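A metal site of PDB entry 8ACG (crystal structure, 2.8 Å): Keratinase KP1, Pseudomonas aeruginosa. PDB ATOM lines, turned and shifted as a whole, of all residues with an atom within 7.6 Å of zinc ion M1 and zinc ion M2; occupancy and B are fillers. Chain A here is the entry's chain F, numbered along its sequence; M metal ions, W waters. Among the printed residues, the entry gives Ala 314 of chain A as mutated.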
ATOM      1  N   HIS A 270     -26.498 -23.810   2.178  1.00  0.00           N
ATOM      2  CA  HIS A 270     -25.621 -22.839   2.824  1.00  0.00           C
ATOM      3  C   HIS A 270     -26.410 -21.572   3.072  1.00  0.00           C
ATOM      4  O   HIS A 270     -27.199 -21.142   2.216  1.00  0.00           O
ATOM      5  CB  HIS A 270     -24.357 -22.550   1.995  1.00  0.00           C
ATOM      6  CG  HIS A 270     -24.547 -21.662   0.796  1.00  0.00           C
ATOM      7  ND1 HIS A 270     -24.459 -20.287   0.859  1.00  0.00           N
ATOM      8  CD2 HIS A 270     -24.762 -21.962  -0.511  1.00  0.00           C
ATOM      9  CE1 HIS A 270     -24.643 -19.776  -0.339  1.00  0.00           C
ATOM     10  NE2 HIS A 270     -24.823 -20.773  -1.194  1.00  0.00           N
ATOM     11  N   ASP A 272     -25.193 -18.427   4.292  1.00  0.00           N
ATOM     12  CA  ASP A 272     -24.583 -17.119   4.086  1.00  0.00           C
ATOM     13  C   ASP A 272     -24.729 -16.654   2.637  1.00  0.00           C
ATOM     14  O   ASP A 272     -24.950 -17.458   1.722  1.00  0.00           O
ATOM     15  CB  ASP A 272     -23.115 -17.133   4.429  1.00  0.00           C
ATOM     16  CG  ASP A 272     -22.329 -18.028   3.492  1.00  0.00           C
ATOM     17  OD1 ASP A 272     -22.796 -19.173   3.309  1.00  0.00           O
ATOM     18  OD2 ASP A 272     -21.315 -17.554   2.909  1.00  0.00           O
ATOM     19  N   SER A 273     -24.552 -15.356   2.444  1.00  0.00           N
ATOM     20  CA  SER A 273     -24.529 -14.725   1.138  1.00  0.00           C
ATOM     21  C   SER A 273     -23.159 -14.096   0.876  1.00  0.00           C
ATOM     22  O   SER A 273     -22.293 -14.036   1.755  1.00  0.00           O
ATOM     23  CB  SER A 273     -25.602 -13.640   1.030  1.00  0.00           C
ATOM     24  OG  SER A 273     -25.225 -12.475   1.774  1.00  0.00           O
ATOM     25  N   VAL A 274     -22.978 -13.611  -0.352  1.00  0.00           N
ATOM     26  CA  VAL A 274     -21.823 -12.785  -0.667  1.00  0.00           C
ATOM     27  C   VAL A 274     -22.018 -11.457   0.044  1.00  0.00           C
ATOM     28  O   VAL A 274     -23.097 -11.189   0.582  1.00  0.00           O
ATOM     29  CB  VAL A 274     -21.622 -12.567  -2.184  1.00  0.00           C
ATOM     30  CG1 VAL A 274     -21.392 -13.857  -2.902  1.00  0.00           C
ATOM     31  CG2 VAL A 274     -22.806 -11.798  -2.760  1.00  0.00           C
ATOM     32  N   ASN A 281     -31.720 -15.782  -3.641  1.00  0.00           N
ATOM     33  CA  ASN A 281     -31.650 -16.998  -4.446  1.00  0.00           C
ATOM     34  C   ASN A 281     -30.412 -17.799  -4.096  1.00  0.00           C
ATOM     35  O   ASN A 281     -30.451 -19.032  -4.019  1.00  0.00           O
ATOM     36  CB  ASN A 281     -31.643 -16.626  -5.929  1.00  0.00           C
ATOM     37  CG  ASN A 281     -31.658 -17.814  -6.831  1.00  0.00           C
ATOM     38  OD1 ASN A 281     -32.301 -18.809  -6.554  1.00  0.00           O
ATOM     39  ND2 ASN A 281     -30.988 -17.710  -7.948  1.00  0.00           N
ATOM     40  N   ASP A 282     -29.276 -17.124  -3.902  1.00  0.00           N
ATOM     41  CA  ASP A 282     -28.027 -17.779  -3.566  1.00  0.00           C
ATOM     42  C   ASP A 282     -27.623 -17.341  -2.165  1.00  0.00           C
ATOM     43  O   ASP A 282     -26.977 -16.302  -2.010  1.00  0.00           O
ATOM     44  CB  ASP A 282     -26.951 -17.449  -4.581  1.00  0.00           C
ATOM     45  CG  ASP A 282     -25.652 -18.137  -4.298  1.00  0.00           C
ATOM     46  OD1 ASP A 282     -25.687 -19.217  -3.677  1.00  0.00           O
ATOM     47  OD2 ASP A 282     -24.595 -17.581  -4.665  1.00  0.00           O
ATOM     48  N   ASN A 283     -27.994 -18.113  -1.147  1.00  0.00           N
ATOM     49  CA  ASN A 283     -28.782 -19.344  -1.253  1.00  0.00           C
ATOM     50  C   ASN A 283     -29.940 -19.264  -0.268  1.00  0.00           C
ATOM     51  O   ASN A 283     -30.162 -20.182   0.507  1.00  0.00           O
ATOM     52  CB  ASN A 283     -27.934 -20.578  -0.940  1.00  0.00           C
ATOM     53  CG  ASN A 283     -28.687 -21.876  -1.103  1.00  0.00           C
ATOM     54  OD1 ASN A 283     -29.532 -22.033  -1.976  1.00  0.00           O
ATOM     55  ND2 ASN A 283     -28.408 -22.814  -0.219  1.00  0.00           N
ATOM     56  N   GLY A 284     -30.655 -18.137  -0.268  1.00  0.00           N
ATOM     57  CA  GLY A 284     -31.863 -18.088   0.526  1.00  0.00           C
ATOM     58  C   GLY A 284     -32.861 -19.136   0.095  1.00  0.00           C
ATOM     59  O   GLY A 284     -33.566 -19.694   0.925  1.00  0.00           O
ATOM     60  N   ALA A 314     -20.030 -20.301   3.261  1.00  0.00           N
ATOM     61  CA  ALA A 314     -19.809 -21.116   2.062  1.00  0.00           C
ATOM     62  C   ALA A 314     -19.235 -20.263   0.954  1.00  0.00           C
ATOM     63  O   ALA A 314     -18.399 -20.750   0.185  1.00  0.00           O
ATOM     64  CB  ALA A 314     -21.080 -21.814   1.602  1.00  0.00           C
ATOM     65  N   GLU A 315     -19.678 -19.002   0.858  1.00  0.00           N
ATOM     66  CA  GLU A 315     -19.155 -18.147  -0.201  1.00  0.00           C
ATOM     67  C   GLU A 315     -17.699 -17.823  -0.006  1.00  0.00           C
ATOM     68  O   GLU A 315     -17.105 -17.178  -0.871  1.00  0.00           O
ATOM     69  CB  GLU A 315     -19.976 -16.845  -0.323  1.00  0.00           C
ATOM     70  CG  GLU A 315     -21.460 -17.098  -0.606  1.00  0.00           C
ATOM     71  CD  GLU A 315     -21.746 -17.606  -2.052  1.00  0.00           C
ATOM     72  OE1 GLU A 315     -20.793 -17.951  -2.768  1.00  0.00           O
ATOM     73  OE2 GLU A 315     -22.908 -17.745  -2.471  1.00  0.00           O
ATOM     74  N   LEU A 318     -16.486 -22.888   0.958  1.00  0.00           N
ATOM     75  CA  LEU A 318     -17.052 -24.082   1.585  1.00  0.00           C
ATOM     76  C   LEU A 318     -16.483 -24.335   2.985  1.00  0.00           C
ATOM     77  O   LEU A 318     -16.239 -25.480   3.383  1.00  0.00           O
ATOM     78  CB  LEU A 318     -16.842 -25.304   0.685  1.00  0.00           C
ATOM     79  CG  LEU A 318     -17.131 -25.160  -0.806  1.00  0.00           C
ATOM     80  CD1 LEU A 318     -16.839 -26.428  -1.563  1.00  0.00           C
ATOM     81  CD2 LEU A 318     -18.526 -24.725  -1.049  1.00  0.00           C
ATOM     82  N   ASN A 341     -27.843 -31.713  -1.313  1.00  0.00           N
ATOM     83  CA  ASN A 341     -27.380 -30.342  -1.284  1.00  0.00           C
ATOM     84  C   ASN A 341     -28.334 -29.527  -2.122  1.00  0.00           C
ATOM     85  O   ASN A 341     -28.647 -29.931  -3.250  1.00  0.00           O
ATOM     86  CB  ASN A 341     -25.945 -30.216  -1.828  1.00  0.00           C
ATOM     87  CG  ASN A 341     -25.326 -28.878  -1.522  1.00  0.00           C
ATOM     88  OD1 ASN A 341     -25.062 -28.595  -0.356  1.00  0.00           O
ATOM     89  ND2 ASN A 341     -25.073 -28.059  -2.536  1.00  0.00           N
ATOM     90  N   PHE A 342     -28.823 -28.405  -1.578  1.00  0.00           N
ATOM     91  CA  PHE A 342     -29.785 -27.564  -2.281  1.00  0.00           C
ATOM     92  C   PHE A 342     -29.285 -26.134  -2.268  1.00  0.00           C
ATOM     93  O   PHE A 342     -29.428 -25.445  -1.262  1.00  0.00           O
ATOM     94  CB  PHE A 342     -31.179 -27.679  -1.693  1.00  0.00           C
ATOM     95  CG  PHE A 342     -31.668 -29.093  -1.659  1.00  0.00           C
ATOM     96  CD1 PHE A 342     -32.095 -29.708  -2.820  1.00  0.00           C
ATOM     97  CD2 PHE A 342     -31.668 -29.819  -0.484  1.00  0.00           C
ATOM     98  CE1 PHE A 342     -32.500 -30.983  -2.808  1.00  0.00           C
ATOM     99  CE2 PHE A 342     -32.084 -31.117  -0.483  1.00  0.00           C
ATOM    100  CZ  PHE A 342     -32.500 -31.690  -1.656  1.00  0.00           C
ATOM    101  N   ASP A 343     -28.689 -25.718  -3.394  1.00  0.00           N
ATOM    102  CA  ASP A 343     -27.970 -24.454  -3.524  1.00  0.00           C
ATOM    103  C   ASP A 343     -28.439 -23.752  -4.801  1.00  0.00           C
ATOM    104  O   ASP A 343     -28.054 -24.159  -5.897  1.00  0.00           O
ATOM    105  CB  ASP A 343     -26.475 -24.709  -3.588  1.00  0.00           C
ATOM    106  CG  ASP A 343     -25.643 -23.460  -3.509  1.00  0.00           C
ATOM    107  OD1 ASP A 343     -26.143 -22.355  -3.814  1.00  0.00           O
ATOM    108  OD2 ASP A 343     -24.457 -23.574  -3.137  1.00  0.00           O
ATOM    109  N   MET A 344     -29.217 -22.672  -4.639  1.00  0.00           N
ATOM    110  CA  MET A 344     -29.804 -21.904  -5.735  1.00  0.00           C
ATOM    111  C   MET A 344     -30.881 -22.678  -6.471  1.00  0.00           C
ATOM    112  O   MET A 344     -30.593 -23.325  -7.478  1.00  0.00           O
ATOM    113  CB  MET A 344     -28.760 -21.457  -6.749  1.00  0.00           C
ATOM    114  CG  MET A 344     -27.919 -20.321  -6.312  1.00  0.00           C
ATOM    115  SD  MET A 344     -26.744 -19.881  -7.593  1.00  0.00           S
ATOM    116  CE  MET A 344     -27.788 -18.989  -8.740  1.00  0.00           C
ATOM    117  N   ARG A 396     -18.191 -27.777  -6.387  1.00  0.00           N
ATOM    118  CA  ARG A 396     -18.554 -26.378  -6.532  1.00  0.00           C
ATOM    119  C   ARG A 396     -19.406 -25.854  -5.372  1.00  0.00           C
ATOM    120  O   ARG A 396     -19.585 -24.626  -5.248  1.00  0.00           O
ATOM    121  CB  ARG A 396     -19.348 -26.229  -7.823  1.00  0.00           C
ATOM    122  CG  ARG A 396     -18.763 -26.886  -9.060  1.00  0.00           C
ATOM    123  CD  ARG A 396     -19.740 -26.639 -10.264  1.00  0.00           C
ATOM    124  NE  ARG A 396     -19.296 -27.156 -11.566  1.00  0.00           N
ATOM    125  CZ  ARG A 396     -18.730 -26.399 -12.516  1.00  0.00           C
ATOM    126  NH1 ARG A 396     -18.345 -26.932 -13.688  1.00  0.00           N
ATOM    127  NH2 ARG A 396     -18.507 -25.110 -12.299  1.00  0.00           N
ATOM    128  N   SER A 397     -19.930 -26.751  -4.531  1.00  0.00           N
ATOM    129  CA  SER A 397     -20.846 -26.368  -3.458  1.00  0.00           C
ATOM    130  C   SER A 397     -20.577 -27.291  -2.266  1.00  0.00           C
ATOM    131  O   SER A 397     -19.635 -28.072  -2.273  1.00  0.00           O
ATOM    132  CB  SER A 397     -22.284 -26.470  -3.966  1.00  0.00           C
ATOM    133  OG  SER A 397     -23.172 -25.954  -3.008  1.00  0.00           O
ATOM    134  N   ASP A 398     -21.431 -27.205  -1.241  1.00  0.00           N
ATOM    135  CA  ASP A 398     -21.145 -27.769   0.077  1.00  0.00           C
ATOM    136  C   ASP A 398     -21.192 -29.281   0.156  1.00  0.00           C
ATOM    137  O   ASP A 398     -20.964 -29.799   1.234  1.00  0.00           O
ATOM    138  CB  ASP A 398     -22.089 -27.199   1.124  1.00  0.00           C
ATOM    139  CG  ASP A 398     -21.901 -25.736   1.296  1.00  0.00           C
ATOM    140  OD1 ASP A 398     -20.848 -25.345   1.873  1.00  0.00           O
ATOM    141  OD2 ASP A 398     -22.756 -24.962   0.828  1.00  0.00           O
ATOM    142  N   PHE A 413     -30.134 -27.705  -8.669  1.00  0.00           N
ATOM    143  CA  PHE A 413     -29.514 -26.469  -9.113  1.00  0.00           C
ATOM    144  C   PHE A 413     -30.418 -25.922 -10.193  1.00  0.00           C
ATOM    145  O   PHE A 413     -30.949 -26.705 -10.999  1.00  0.00           O
ATOM    146  CB  PHE A 413     -28.116 -26.710  -9.673  1.00  0.00           C
ATOM    147  CG  PHE A 413     -27.364 -25.451 -10.029  1.00  0.00           C
ATOM    148  CD1 PHE A 413     -27.399 -24.348  -9.199  1.00  0.00           C
ATOM    149  CD2 PHE A 413     -26.567 -25.401 -11.158  1.00  0.00           C
ATOM    150  CE1 PHE A 413     -26.677 -23.196  -9.513  1.00  0.00           C
ATOM    151  CE2 PHE A 413     -25.837 -24.277 -11.457  1.00  0.00           C
ATOM    152  CZ  PHE A 413     -25.890 -23.169 -10.639  1.00  0.00           C
ATOM    153  N   ALA A 416     -26.704 -20.606 -12.688  1.00  0.00           N
ATOM    154  CA  ALA A 416     -26.152 -19.345 -12.203  1.00  0.00           C
ATOM    155  C   ALA A 416     -25.692 -18.446 -13.329  1.00  0.00           C
ATOM    156  O   ALA A 416     -26.516 -17.819 -13.990  1.00  0.00           O
ATOM    157  CB  ALA A 416     -25.012 -19.579 -11.214  1.00  0.00           C
ATOM    158  N   TYR A 440     -26.845 -12.962 -10.159  1.00  0.00           N
ATOM    159  CA  TYR A 440     -25.947 -13.845  -9.408  1.00  0.00           C
ATOM    160  C   TYR A 440     -24.837 -13.076  -8.697  1.00  0.00           C
ATOM    161  O   TYR A 440     -24.111 -12.286  -9.297  1.00  0.00           O
ATOM    162  CB  TYR A 440     -25.347 -14.854 -10.383  1.00  0.00           C
ATOM    163  CG  TYR A 440     -24.285 -15.741  -9.810  1.00  0.00           C
ATOM    164  CD1 TYR A 440     -24.557 -16.626  -8.780  1.00  0.00           C
ATOM    165  CD2 TYR A 440     -23.010 -15.721 -10.346  1.00  0.00           C
ATOM    166  CE1 TYR A 440     -23.584 -17.455  -8.280  1.00  0.00           C
ATOM    167  CE2 TYR A 440     -22.026 -16.538  -9.862  1.00  0.00           C
ATOM    168  CZ  TYR A 440     -22.301 -17.402  -8.820  1.00  0.00           C
ATOM    169  OH  TYR A 440     -21.308 -18.227  -8.330  1.00  0.00           O
ATOM    170  N   HIS A 441     -24.752 -13.315  -7.394  1.00  0.00           N
ATOM    171  CA  HIS A 441     -23.760 -12.707  -6.526  1.00  0.00           C
ATOM    172  C   HIS A 441     -23.828 -11.188  -6.576  1.00  0.00           C
ATOM    173  O   HIS A 441     -22.847 -10.510  -6.285  1.00  0.00           O
ATOM    174  CB  HIS A 441     -22.353 -13.199  -6.831  1.00  0.00           C
ATOM    175  CG  HIS A 441     -22.104 -14.584  -6.342  1.00  0.00           C
ATOM    176  ND1 HIS A 441     -20.883 -15.219  -6.476  1.00  0.00           N
ATOM    177  CD2 HIS A 441     -22.918 -15.463  -5.716  1.00  0.00           C
ATOM    178  CE1 HIS A 441     -20.955 -16.425  -5.932  1.00  0.00           C
ATOM    179  NE2 HIS A 441     -22.180 -16.602  -5.475  1.00  0.00           N
HETATM  180 ZN    ZN M   1     -24.557 -21.001  -3.662  1.00  0.00          ZN
HETATM  181 ZN    ZN M   2     -22.554 -18.582  -4.601  1.00  0.00          ZN
HETATM  182  O   HOH W   1     -23.432 -20.672  -6.608  1.00  0.00           O
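Zinc ion M2 is bound by NE2 of His 441 (2.2 Å). The side-chain carboxylate (OD2) of Asp 282 binds zinc ion M2 (2.3 Å). OE2 of Glu 315 binds zinc ion M2 (2.3 Å). Slightly farther from zinc ion M2 lies OE1 of Glu 315 (2.6 Å).
Zinc ion M1 is bound by OD1 of Asp 343, OD1 of Asp 282 and NE2 of His 270. Zinc ion M1 has three donor atoms within binding distance. Slightly farther from zinc ion M1 lies OD2 of Asp 343 (2.6 Å).
The side-chain amide nitrogen of Asn 283 is in hydrogen-bond range of the backbone carbonyl oxygen of His 270, 3.2 Å away. OH of Tyr 440 sits close to NE2 of His 441 (3.4 Å). O of Asp 272 lies within hydrogen-bond range of ND1 of His 270 (3.0 Å). OD2 of Asp 343 sits at hydrogen-bond distance from OG of Ser 397 (2.7 Å). The backbone NH (N) of Glu 315 is in hydrogen-bond range of the side-chain carboxylate (OD2) of Asp 272 (3.0 Å).
Of the 22 residues printed, 4 come within 4 Å of zinc ion M1.
Merely in contact with zinc ion M2: Tyr 440 (3.9 Å).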
